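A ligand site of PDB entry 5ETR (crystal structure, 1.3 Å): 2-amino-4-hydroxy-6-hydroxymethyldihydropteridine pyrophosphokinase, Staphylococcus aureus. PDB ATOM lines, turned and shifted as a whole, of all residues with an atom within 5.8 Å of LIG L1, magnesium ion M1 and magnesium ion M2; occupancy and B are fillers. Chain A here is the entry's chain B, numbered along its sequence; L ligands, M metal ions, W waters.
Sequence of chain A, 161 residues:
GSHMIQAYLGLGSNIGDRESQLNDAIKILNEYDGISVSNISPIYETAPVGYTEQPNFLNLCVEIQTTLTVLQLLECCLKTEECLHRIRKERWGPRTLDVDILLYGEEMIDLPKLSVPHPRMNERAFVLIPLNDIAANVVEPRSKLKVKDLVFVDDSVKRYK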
ATOM      1  N   LEU A  74      10.098   3.313  24.002  1.00  0.00           N
ATOM      2  CA  LEU A  74      11.050   4.411  23.975  1.00  0.00           C
ATOM      3  C   LEU A  74      12.466   3.871  23.953  1.00  0.00           C
ATOM      4  O   LEU A  74      13.301   4.330  23.176  1.00  0.00           O
ATOM      5  CB  LEU A  74      10.856   5.317  25.187  1.00  0.00           C
ATOM      6  CG  LEU A  74      11.932   6.393  25.330  1.00  0.00           C
ATOM      7  CD1 LEU A  74      11.840   7.402  24.195  1.00  0.00           C
ATOM      8  CD2 LEU A  74      11.825   7.082  26.683  1.00  0.00           C
ATOM      9  N   LEU A  78      15.279   4.817  21.005  1.00  0.00           N
ATOM     10  CA  LEU A  78      16.608   5.398  21.289  1.00  0.00           C
ATOM     11  C   LEU A  78      17.752   4.472  20.901  1.00  0.00           C
ATOM     12  O   LEU A  78      18.766   4.934  20.373  1.00  0.00           O
ATOM     13  CB  LEU A  78      16.687   5.791  22.771  1.00  0.00           C
ATOM     14  CG  LEU A  78      15.629   6.764  23.272  1.00  0.00           C
ATOM     15  CD1 LEU A  78      15.846   7.074  24.762  1.00  0.00           C
ATOM     16  CD2 LEU A  78      15.617   8.069  22.476  1.00  0.00           C
ATOM     17  N   GLU A  81      18.384   4.985  17.187  1.00  0.00           N
ATOM     18  CA  GLU A  81      19.217   6.168  16.969  1.00  0.00           C
ATOM     19  C   GLU A  81      20.698   5.830  17.156  1.00  0.00           C
ATOM     20  O   GLU A  81      21.572   6.309  16.402  1.00  0.00           O
ATOM     21  CB  GLU A  81      18.809   7.283  17.876  1.00  0.00           C
ATOM     22  CG  GLU A  81      17.414   7.850  17.608  1.00  0.00           C
ATOM     23  CD  GLU A  81      16.982   8.888  18.618  1.00  0.00           C
ATOM     24  OE1 GLU A  81      17.649   8.982  19.670  1.00  0.00           O
ATOM     25  OE2 GLU A  81      15.951   9.534  18.355  1.00  0.00           O
ATOM     26  N   ARG A  86      23.928   8.418  15.878  1.00  0.00           N
ATOM     27  CA  ARG A  86      23.609   9.802  16.202  1.00  0.00           C
ATOM     28  C   ARG A  86      24.559  10.402  17.227  1.00  0.00           C
ATOM     29  O   ARG A  86      24.847   9.791  18.209  1.00  0.00           O
ATOM     30  CB  ARG A  86      22.194   9.850  16.718  1.00  0.00           C
ATOM     31  CG  ARG A  86      21.843  11.257  17.201  1.00  0.00           C
ATOM     32  CD  ARG A  86      20.354  11.394  17.386  1.00  0.00           C
ATOM     33  NE  ARG A  86      19.968  12.640  18.041  1.00  0.00           N
ATOM     34  CZ  ARG A  86      18.704  12.953  18.254  1.00  0.00           C
ATOM     35  NH1 ARG A  86      17.740  12.172  17.826  1.00  0.00           N
ATOM     36  NH2 ARG A  86      18.394  14.085  18.878  1.00  0.00           N
ATOM     37  N   ARG A  88      25.566  13.338  19.982  1.00  0.00           N
ATOM     38  CA  ARG A  88      24.910  14.189  20.994  1.00  0.00           C
ATOM     39  C   ARG A  88      25.973  15.067  21.640  1.00  0.00           C
ATOM     40  O   ARG A  88      26.723  14.615  22.524  1.00  0.00           O
ATOM     41  CB  ARG A  88      24.177  13.283  21.976  1.00  0.00           C
ATOM     42  CG  ARG A  88      23.375  12.126  21.383  1.00  0.00           C
ATOM     43  CD  ARG A  88      22.653  11.428  22.488  1.00  0.00           C
ATOM     44  NE  ARG A  88      21.691  12.385  23.011  1.00  0.00           N
ATOM     45  CZ  ARG A  88      20.497  12.552  22.470  1.00  0.00           C
ATOM     46  NH1 ARG A  88      19.678  13.471  22.956  1.00  0.00           N
ATOM     47  NH2 ARG A  88      20.114  11.755  21.450  1.00  0.00           N
ATOM     48  N   ARG A  95      21.244  15.666  12.805  1.00  0.00           N
ATOM     49  CA  ARG A  95      21.270  14.314  13.363  1.00  0.00           C
ATOM     50  C   ARG A  95      20.977  13.316  12.256  1.00  0.00           C
ATOM     51  O   ARG A  95      20.143  13.510  11.389  1.00  0.00           O
ATOM     52  CB  ARG A  95      20.344  14.125  14.530  1.00  0.00           C
ATOM     53  CG  ARG A  95      18.867  14.248  14.305  1.00  0.00           C
ATOM     54  CD  ARG A  95      18.328  15.671  14.033  1.00  0.00           C
ATOM     55  NE  ARG A  95      18.713  16.545  15.133  1.00  0.00           N
ATOM     56  CZ  ARG A  95      18.041  16.684  16.281  1.00  0.00           C
ATOM     57  NH1 ARG A  95      16.795  16.228  16.429  1.00  0.00           N
ATOM     58  NH2 ARG A  95      18.647  17.307  17.307  1.00  0.00           N
ATOM     59  N   ASP A  98      16.329  10.712  14.191  1.00  0.00           N
ATOM     60  CA  ASP A  98      15.498  11.039  15.361  1.00  0.00           C
ATOM     61  C   ASP A  98      14.250  10.191  15.272  1.00  0.00           C
ATOM     62  O   ASP A  98      13.593  10.222  14.247  1.00  0.00           O
ATOM     63  CB  ASP A  98      15.134  12.543  15.322  1.00  0.00           C
ATOM     64  CG  ASP A  98      14.365  13.034  16.546  1.00  0.00           C
ATOM     65  OD1 ASP A  98      14.700  12.603  17.658  1.00  0.00           O
ATOM     66  OD2 ASP A  98      13.372  13.848  16.355  1.00  0.00           O
ATOM     67  N   VAL A  99      13.976   9.455  16.340  1.00  0.00           N
ATOM     68  CA  VAL A  99      12.757   8.617  16.469  1.00  0.00           C
ATOM     69  C   VAL A  99      11.968   9.094  17.654  1.00  0.00           C
ATOM     70  O   VAL A  99      12.388   8.868  18.792  1.00  0.00           O
ATOM     71  CB  VAL A  99      13.086   7.109  16.591  1.00  0.00           C
ATOM     72  CG1 VAL A  99      11.798   6.334  16.506  1.00  0.00           C
ATOM     73  CG2 VAL A  99      14.061   6.637  15.514  1.00  0.00           C
ATOM     74  N   ASP A 100      10.812   9.703  17.355  1.00  0.00           N
ATOM     75  CA  ASP A 100       9.967  10.304  18.403  1.00  0.00           C
ATOM     76  C   ASP A 100       8.661   9.538  18.510  1.00  0.00           C
ATOM     77  O   ASP A 100       8.047   9.201  17.490  1.00  0.00           O
ATOM     78  CB  ASP A 100       9.682  11.758  18.085  1.00  0.00           C
ATOM     79  CG  ASP A 100      10.905  12.649  18.180  1.00  0.00           C
ATOM     80  OD1 ASP A 100      11.942  12.198  18.735  1.00  0.00           O
ATOM     81  OD2 ASP A 100      10.776  13.827  17.728  1.00  0.00           O
ATOM     82  N   ILE A 101       8.216   9.248  19.745  1.00  0.00           N
ATOM     83  CA  ILE A 101       6.896   8.635  19.935  1.00  0.00           C
ATOM     84  C   ILE A 101       5.885   9.756  19.855  1.00  0.00           C
ATOM     85  O   ILE A 101       5.884  10.685  20.664  1.00  0.00           O
ATOM     86  CB  ILE A 101       6.793   7.862  21.239  1.00  0.00           C
ATOM     87  CG1 ILE A 101       7.849   6.753  21.340  1.00  0.00           C
ATOM     88  CG2 ILE A 101       5.390   7.356  21.393  1.00  0.00           C
ATOM     89  CD1 ILE A 101       7.977   6.156  22.723  1.00  0.00           C
ATOM     90  N   LEU A 102       4.993   9.683  18.865  1.00  0.00           N
ATOM     91  CA  LEU A 102       3.951  10.699  18.691  1.00  0.00           C
ATOM     92  C   LEU A 102       2.709  10.386  19.496  1.00  0.00           C
ATOM     93  O   LEU A 102       2.189  11.229  20.224  1.00  0.00           O
ATOM     94  CB  LEU A 102       3.648  10.872  17.214  1.00  0.00           C
ATOM     95  CG  LEU A 102       4.839  11.261  16.305  1.00  0.00           C
ATOM     96  CD1 LEU A 102       4.421  11.229  14.853  1.00  0.00           C
ATOM     97  CD2 LEU A 102       5.432  12.592  16.741  1.00  0.00           C
ATOM     98  N   PRO A 112       9.327  12.387  33.511  1.00  0.00           N
ATOM     99  CA  PRO A 112      10.492  13.194  33.181  1.00  0.00           C
ATOM    100  C   PRO A 112      11.110  12.796  31.856  1.00  0.00           C
ATOM    101  O   PRO A 112      11.586  13.646  31.094  1.00  0.00           O
ATOM    102  CB  PRO A 112      11.398  12.968  34.399  1.00  0.00           C
ATOM    103  CG  PRO A 112      10.438  12.780  35.495  1.00  0.00           C
ATOM    104  CD  PRO A 112       9.343  11.964  34.934  1.00  0.00           C
ATOM    105  N   LYS A 113      11.215  11.507  31.555  1.00  0.00           N
ATOM    106  CA  LYS A 113      11.899  11.066  30.344  1.00  0.00           C
ATOM    107  C   LYS A 113      10.939  10.823  29.187  1.00  0.00           C
ATOM    108  O   LYS A 113      11.409  10.410  28.118  1.00  0.00           O
ATOM    109  CB  LYS A 113      12.737   9.781  30.575  1.00  0.00           C
ATOM    110  CG  LYS A 113      11.994   8.457  30.908  1.00  0.00           C
ATOM    111  CD  LYS A 113      12.840   7.243  31.468  1.00  0.00           C
ATOM    112  CE  LYS A 113      13.842   6.653  30.487  1.00  0.00           C
ATOM    113  NZ  LYS A 113      14.598   5.550  31.166  1.00  0.00           N
ATOM    114  N   LEU A 114       9.627  11.020  29.343  1.00  0.00           N
ATOM    115  CA  LEU A 114       8.693  10.637  28.280  1.00  0.00           C
ATOM    116  C   LEU A 114       7.419  11.446  28.369  1.00  0.00           C
ATOM    117  O   LEU A 114       6.687  11.343  29.395  1.00  0.00           O
ATOM    118  CB  LEU A 114       8.381   9.123  28.353  1.00  0.00           C
ATOM    119  CG  LEU A 114       7.476   8.591  27.262  1.00  0.00           C
ATOM    120  CD1 LEU A 114       7.980   8.843  25.856  1.00  0.00           C
ATOM    121  CD2 LEU A 114       7.160   7.137  27.523  1.00  0.00           C
ATOM    122  N   SER A 115       7.079  12.133  27.283  1.00  0.00           N
ATOM    123  CA  SER A 115       5.806  12.871  27.176  1.00  0.00           C
ATOM    124  C   SER A 115       5.117  12.404  25.903  1.00  0.00           C
ATOM    125  O   SER A 115       5.663  12.576  24.811  1.00  0.00           O
ATOM    126  CB  SER A 115       6.070  14.375  27.107  1.00  0.00           C
ATOM    127  OG  SER A 115       6.771  14.837  28.237  1.00  0.00           O
ATOM    128  N   VAL A 116       3.931  11.822  26.058  1.00  0.00           N
ATOM    129  CA  VAL A 116       3.135  11.323  24.948  1.00  0.00           C
ATOM    130  C   VAL A 116       1.667  11.722  25.195  1.00  0.00           C
ATOM    131  O   VAL A 116       1.207  11.508  26.326  1.00  0.00           O
ATOM    132  CB  VAL A 116       3.221   9.785  24.845  1.00  0.00           C
ATOM    133  CG1 VAL A 116       2.319   9.261  23.699  1.00  0.00           C
ATOM    134  CG2 VAL A 116       4.666   9.340  24.612  1.00  0.00           C
ATOM    135  N   PRO A 117       0.923  12.214  24.204  1.00  0.00           N
ATOM    136  CA  PRO A 117       1.393  12.602  22.889  1.00  0.00           C
ATOM    137  C   PRO A 117       2.571  13.527  22.905  1.00  0.00           C
ATOM    138  O   PRO A 117       2.759  14.312  23.857  1.00  0.00           O
ATOM    139  CB  PRO A 117       0.172  13.261  22.276  1.00  0.00           C
ATOM    140  CG  PRO A 117      -0.958  12.583  22.966  1.00  0.00           C
ATOM    141  CD  PRO A 117      -0.529  12.448  24.373  1.00  0.00           C
ATOM    142  N   HIS A 118       3.386  13.519  21.854  1.00  0.00           N
ATOM    143  CA  HIS A 118       4.545  14.349  21.810  1.00  0.00           C
ATOM    144  C   HIS A 118       4.123  15.812  22.027  1.00  0.00           C
ATOM    145  O   HIS A 118       3.184  16.272  21.388  1.00  0.00           O
ATOM    146  CB  HIS A 118       5.290  14.185  20.479  1.00  0.00           C
ATOM    147  CG  HIS A 118       6.587  14.896  20.434  1.00  0.00           C
ATOM    148  ND1 HIS A 118       6.678  16.271  20.379  1.00  0.00           N
ATOM    149  CD2 HIS A 118       7.843  14.443  20.604  1.00  0.00           C
ATOM    150  CE1 HIS A 118       7.943  16.600  20.451  1.00  0.00           C
ATOM    151  NE2 HIS A 118       8.681  15.502  20.566  1.00  0.00           N
ATOM    152  N   PRO A 119       4.816  16.559  22.913  1.00  0.00           N
ATOM    153  CA  PRO A 119       4.306  17.865  23.323  1.00  0.00           C
ATOM    154  C   PRO A 119       4.237  18.896  22.281  1.00  0.00           C
ATOM    155  O   PRO A 119       3.581  19.927  22.488  1.00  0.00           O
ATOM    156  CB  PRO A 119       5.217  18.269  24.427  1.00  0.00           C
ATOM    157  CG  PRO A 119       6.264  17.326  24.512  1.00  0.00           C
ATOM    158  CD  PRO A 119       5.956  16.122  23.748  1.00  0.00           C
ATOM    159  N   ARG A 120       4.940  18.726  21.172  1.00  0.00           N
ATOM    160  CA  ARG A 120       4.980  19.705  20.098  1.00  0.00           C
ATOM    161  C   ARG A 120       4.273  19.303  18.821  1.00  0.00           C
ATOM    162  O   ARG A 120       4.227  20.074  17.875  1.00  0.00           O
ATOM    163  CB  ARG A 120       6.455  20.099  19.831  1.00  0.00           C
ATOM    164  CG  ARG A 120       7.068  20.949  20.953  1.00  0.00           C
ATOM    165  CD  ARG A 120       8.578  21.092  20.923  1.00  0.00           C
ATOM    166  NE  ARG A 120       9.302  19.900  21.350  1.00  0.00           N
ATOM    167  CZ  ARG A 120       9.438  19.554  22.616  1.00  0.00           C
ATOM    168  NH1 ARG A 120       8.863  20.247  23.623  1.00  0.00           N
ATOM    169  NH2 ARG A 120      10.080  18.458  22.929  1.00  0.00           N
ATOM    170  N   ARG A 124       3.264  21.174  14.524  1.00  0.00           N
ATOM    171  CA  ARG A 124       4.355  20.820  13.599  1.00  0.00           C
ATOM    172  C   ARG A 124       3.830  20.244  12.315  1.00  0.00           C
ATOM    173  O   ARG A 124       3.369  19.101  12.303  1.00  0.00           O
ATOM    174  CB  ARG A 124       5.320  19.821  14.225  1.00  0.00           C
ATOM    175  CG  ARG A 124       6.230  20.486  15.239  1.00  0.00           C
ATOM    176  CD  ARG A 124       7.008  19.511  16.070  1.00  0.00           C
ATOM    177  NE  ARG A 124       8.178  20.120  16.679  1.00  0.00           N
ATOM    178  CZ  ARG A 124       9.156  19.460  17.275  1.00  0.00           C
ATOM    179  NH1 ARG A 124       9.086  18.132  17.423  1.00  0.00           N
ATOM    180  NH2 ARG A 124      10.224  20.130  17.685  1.00  0.00           N
ATOM    181  N   PHE A 126       5.681  19.223   9.883  1.00  0.00           N
ATOM    182  CA  PHE A 126       6.528  18.096   9.502  1.00  0.00           C
ATOM    183  C   PHE A 126       6.094  16.815  10.196  1.00  0.00           C
ATOM    184  O   PHE A 126       6.514  15.714   9.743  1.00  0.00           O
ATOM    185  CB  PHE A 126       7.999  18.380   9.756  1.00  0.00           C
ATOM    186  CG  PHE A 126       8.441  18.315  11.208  1.00  0.00           C
ATOM    187  CD1 PHE A 126       8.739  17.106  11.766  1.00  0.00           C
ATOM    188  CD2 PHE A 126       8.645  19.489  11.957  1.00  0.00           C
ATOM    189  CE1 PHE A 126       9.188  17.026  13.092  1.00  0.00           C
ATOM    190  CE2 PHE A 126       9.127  19.421  13.241  1.00  0.00           C
ATOM    191  CZ  PHE A 126       9.395  18.197  13.817  1.00  0.00           C
HETATM  192  P1  LIG L   1      11.730  17.281  19.843  1.00  0.00           P
HETATM  193  O1  LIG L   1      11.336  16.628  18.532  1.00  0.00           O
HETATM  194  O2  LIG L   1      11.208  16.588  21.014  1.00  0.00           O
HETATM  195  O3  LIG L   1      11.459  18.758  19.925  1.00  0.00           O
HETATM  196  P2  LIG L   1      14.294  15.908  19.835  1.00  0.00           P
HETATM  197  O4  LIG L   1      13.478  14.789  19.211  1.00  0.00           O
HETATM  198  O5  LIG L   1      15.513  16.315  19.076  1.00  0.00           O
HETATM  199  O6  LIG L   1      13.373  17.177  19.988  1.00  0.00           O
HETATM  200  P3  LIG L   1      15.872  14.100  21.574  1.00  0.00           P
HETATM  201  O7  LIG L   1      15.599  13.179  20.434  1.00  0.00           O
HETATM  202  O8  LIG L   1      17.253  14.586  21.724  1.00  0.00           O
HETATM  203  C1  LIG L   1      14.725  15.492  21.535  1.00  0.00           C
HETATM  204  O9  LIG L   1      15.459  13.235  22.835  1.00  0.00           O
HETATM  205  C2  LIG L   1      15.767  13.721  24.155  1.00  0.00           C
HETATM  206  C3  LIG L   1      14.926  12.931  25.135  1.00  0.00           C
HETATM  207  O10 LIG L   1      13.523  13.183  24.911  1.00  0.00           O
HETATM  208  C4  LIG L   1      14.958  11.380  25.067  1.00  0.00           C
HETATM  209  O11 LIG L   1      16.080  10.816  25.681  1.00  0.00           O
HETATM  210  C5  LIG L   1      13.653  10.954  25.775  1.00  0.00           C
HETATM  211  O12 LIG L   1      13.905  10.518  27.134  1.00  0.00           O
HETATM  212  C6  LIG L   1      12.821  12.235  25.748  1.00  0.00           C
HETATM  213  N1  LIG L   1      11.466  12.120  25.245  1.00  0.00           N
HETATM  214  C7  LIG L   1      10.359  12.673  25.861  1.00  0.00           C
HETATM  215  N2  LIG L   1       9.224  12.456  25.225  1.00  0.00           N
HETATM  216  C8  LIG L   1       9.634  11.733  24.114  1.00  0.00           C
HETATM  217  C9  LIG L   1       8.916  11.213  23.040  1.00  0.00           C
HETATM  218  N3  LIG L   1       7.544  11.381  22.898  1.00  0.00           N
HETATM  219  N4  LIG L   1       9.581  10.483  22.101  1.00  0.00           N
HETATM  220  C10 LIG L   1      10.910  10.349  22.202  1.00  0.00           C
HETATM  221  N5  LIG L   1      11.682  10.807  23.197  1.00  0.00           N
HETATM  222  C11 LIG L   1      10.989  11.484  24.121  1.00  0.00           C
HETATM  223  C1  LG2 L   2      17.261  20.569  16.188  1.00  0.00           C
HETATM  224  C2  LG2 L   2      16.240  21.860  14.505  1.00  0.00           C
HETATM  225  C3  LG2 L   2      18.329  20.239  15.365  1.00  0.00           C
HETATM  226  C4  LG2 L   2      17.279  21.519  13.656  1.00  0.00           C
HETATM  227  C5  LG2 L   2      16.217  21.363  15.802  1.00  0.00           C
HETATM  228  C6  LG2 L   2      18.293  20.749  14.093  1.00  0.00           C
HETATM  229  C7  LG2 L   2      12.714  18.710  13.683  1.00  0.00           C
HETATM  230  C8  LG2 L   2      12.598  20.036  13.380  1.00  0.00           C
HETATM  231  C9  LG2 L   2      13.227  19.732  15.458  1.00  0.00           C
HETATM  232  C10 LG2 L   2      12.373  17.750  12.666  1.00  0.00           C
HETATM  233  C11 LG2 L   2      11.961  19.708  11.271  1.00  0.00           C
HETATM  234  C12 LG2 L   2      15.026  21.639  16.747  1.00  0.00           C
HETATM  235  N1  LG2 L   2      13.126  18.513  14.977  1.00  0.00           N
HETATM  236  N2  LG2 L   2      12.281  20.586  12.222  1.00  0.00           N
HETATM  237  N3  LG2 L   2      12.959  20.690  14.514  1.00  0.00           N
HETATM  238  N4  LG2 L   2      12.023  18.350  11.479  1.00  0.00           N
HETATM  239  N5  LG2 L   2      11.565  20.079  10.057  1.00  0.00           N
HETATM  240  O1  LG2 L   2      12.377  16.494  12.758  1.00  0.00           O
HETATM  241  F1  LG2 L   2      19.313  20.427  13.260  1.00  0.00           F
HETATM  242  S1  LG2 L   2      13.744  20.119  17.085  1.00  0.00           S
HETATM  243 MG    MG M   1      13.777  12.752  19.509  1.00  0.00          MG
HETATM  244 MG    MG M   2      12.307  15.217  17.464  1.00  0.00          MG
HETATM  245  O   HOH W   1      13.791  15.500  27.342  1.00  0.00           O
HETATM  246  O   HOH W   2      12.850  12.825  21.388  1.00  0.00           O
HETATM  247  O   HOH W   3      18.461  17.013  21.597  1.00  0.00           O
HETATM  248  O   HOH W   4      11.404  14.655  22.810  1.00  0.00           O
HETATM  249  O   HOH W   5      14.107  10.734  19.888  1.00  0.00           O
HETATM  250  O   HOH W   6      16.039   8.739  27.989  1.00  0.00           O
HETATM  251  O   HOH W   7      13.715  16.643  16.848  1.00  0.00           O
HETATM  252  O   HOH W   8      11.185  14.411  28.420  1.00  0.00           O
HETATM  253  O   HOH W   9      18.024  10.754  23.877  1.00  0.00           O
HETATM  254  O   HOH W  10      17.289  11.091  21.270  1.00  0.00           O
HETATM  255  O   HOH W  11      17.186  18.279  19.617  1.00  0.00           O
HETATM  256  O   HOH W  12      16.049  12.180  28.581  1.00  0.00           O
HETATM  257  O   HOH W  13      13.161  19.992  21.514  1.00  0.00           O
HETATM  258  O   HOH W  14      12.801  16.131  24.872  1.00  0.00           O
HETATM  259  O   HOH W  15       8.989  15.101  24.125  1.00  0.00           O
HETATM  260  O   HOH W  16      11.340  15.749  15.650  1.00  0.00           O
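Two residues have an atom within 4 Å of magnesium ion M2: Asp 98 and Asp 100.
The nearest printed residue that does not touch magnesium ion M2 is Arg 124 (4.3 Å).
Magnesium ion M1 is bound by the side-chain carboxylate (OD1) of Asp 100 (2.1 Å), the side-chain carboxylate (OD1) of Asp 98 (2.1 Å), water W5 (2.1 Å), an oxygen (O4) of LIG L1 (2.1 Å), an oxygen (O7) of LIG L1 (2.1 Å) and water W2 (2.1 Å).
Magnesium ion M1 has six donor atoms within binding distance.
The side-chain carboxylate (OD1) of Asp 98 sits close to the guanidinium group (NH1) of Arg 86.
The backbone NH (N) of His 118 is in hydrogen-bond range of the backbone carbonyl oxygen (O) of Leu 102 (3.1 Å).
A ring nitrogen (ND1) of His 118 sits at hydrogen-bond distance from the backbone NH of Arg 120 (3.1 Å).
The guanidinium group (NH1) of Arg 86 lies within salt-bridge range of the side-chain carboxylate (OE2) of Glu 81, 3.2 Å away.
Water W5 lies within hydrogen-bond range of OE2 of Glu 81 (2.7 Å) and O of Val 99 (2.8 Å).
Water W7 lies within hydrogen-bond range of a nitrogen (N1) of LG2 L2 (2.7 Å), an oxygen (O5) of LIG L1 (2.9 Å) and the guanidinium group of Arg 95 (3.1 Å).
Water W11 bridges O5 of LIG L1 (2.6 Å) and NH2 of Arg 95 (2.9 Å).
Water W9 lies within hydrogen-bond range of an oxygen (O11) of LIG L1 and the guanidinium group (NH1) of Arg 88.
Water W10 lies within hydrogen-bond range of the side-chain carboxylate of Glu 81 (2.7 Å), the guanidinium group of Arg 88 (2.9 Å) and an oxygen (O9) of LIG L1 (3.2 Å).
Magnesium ion M2 is bound by O1 of LIG L1 (2.0 Å), OD2 of Asp 98 (2.1 Å), OD2 of Asp 100 (2.1 Å), water W7 (2.1 Å), water W16 (2.1 Å) and O4 of LIG L1 (2.1 Å).
Merely in contact with LIG L1: Leu 74, Leu 114, Leu 78 and Val 116.
Hydrophobic or aromatic side chains within 4 Å of LIG L1: Leu 74, Leu 78, Ile 101, Leu 114, Val 116 and His 118.
15 residues have an atom within 4 Å of LIG L1: Leu 74, Leu 78, Arg 86, Arg 88, Arg 95, Asp 98, Asp 100, Ile 101, Lys 113, Leu 114, Ser 115, Val 116, His 118, Arg 120 and Arg 124.
The nearest printed residue that does not touch LIG L1 is Val 99 (4.001 Å).
S1 of LG2 L2 sits close to NH2 of Arg 124 (3.6 Å).
O of Lys 113 lies within hydrogen-bond range of O12 of LIG L1 (2.7 Å).
O8 of LIG L1 lies within salt-bridge range of NH2 of Arg 86, at 3.1 Å.
N of Ser 115 sits at hydrogen-bond distance from N2 of LIG L1 (3.0 Å).
A ring nitrogen (NE2) of His 118 is in hydrogen-bond range of an oxygen (O2) of LIG L1 (2.8 Å).
NH1 of Arg 88 is in salt-bridge range of O8 of LIG L1, at 2.9 Å.
The guanidinium group (NH1) of Arg 95 is in salt-bridge range of an oxygen (O5) of LIG L1 (2.9 Å).
N3 of LIG L1 sits at hydrogen-bond distance from O of Ser 115 (2.9 Å).
O of Ile 101 sits at hydrogen-bond distance from N3 of LIG L1 (2.9 Å).
N of Ile 101 is in hydrogen-bond range of N4 of LIG L1, at 3.0 Å.
O3 of LIG L1 lies within salt-bridge range of NE of Arg 120 (2.8 Å).
NH2 of Arg 124 lies within salt-bridge range of O3 of LIG L1.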
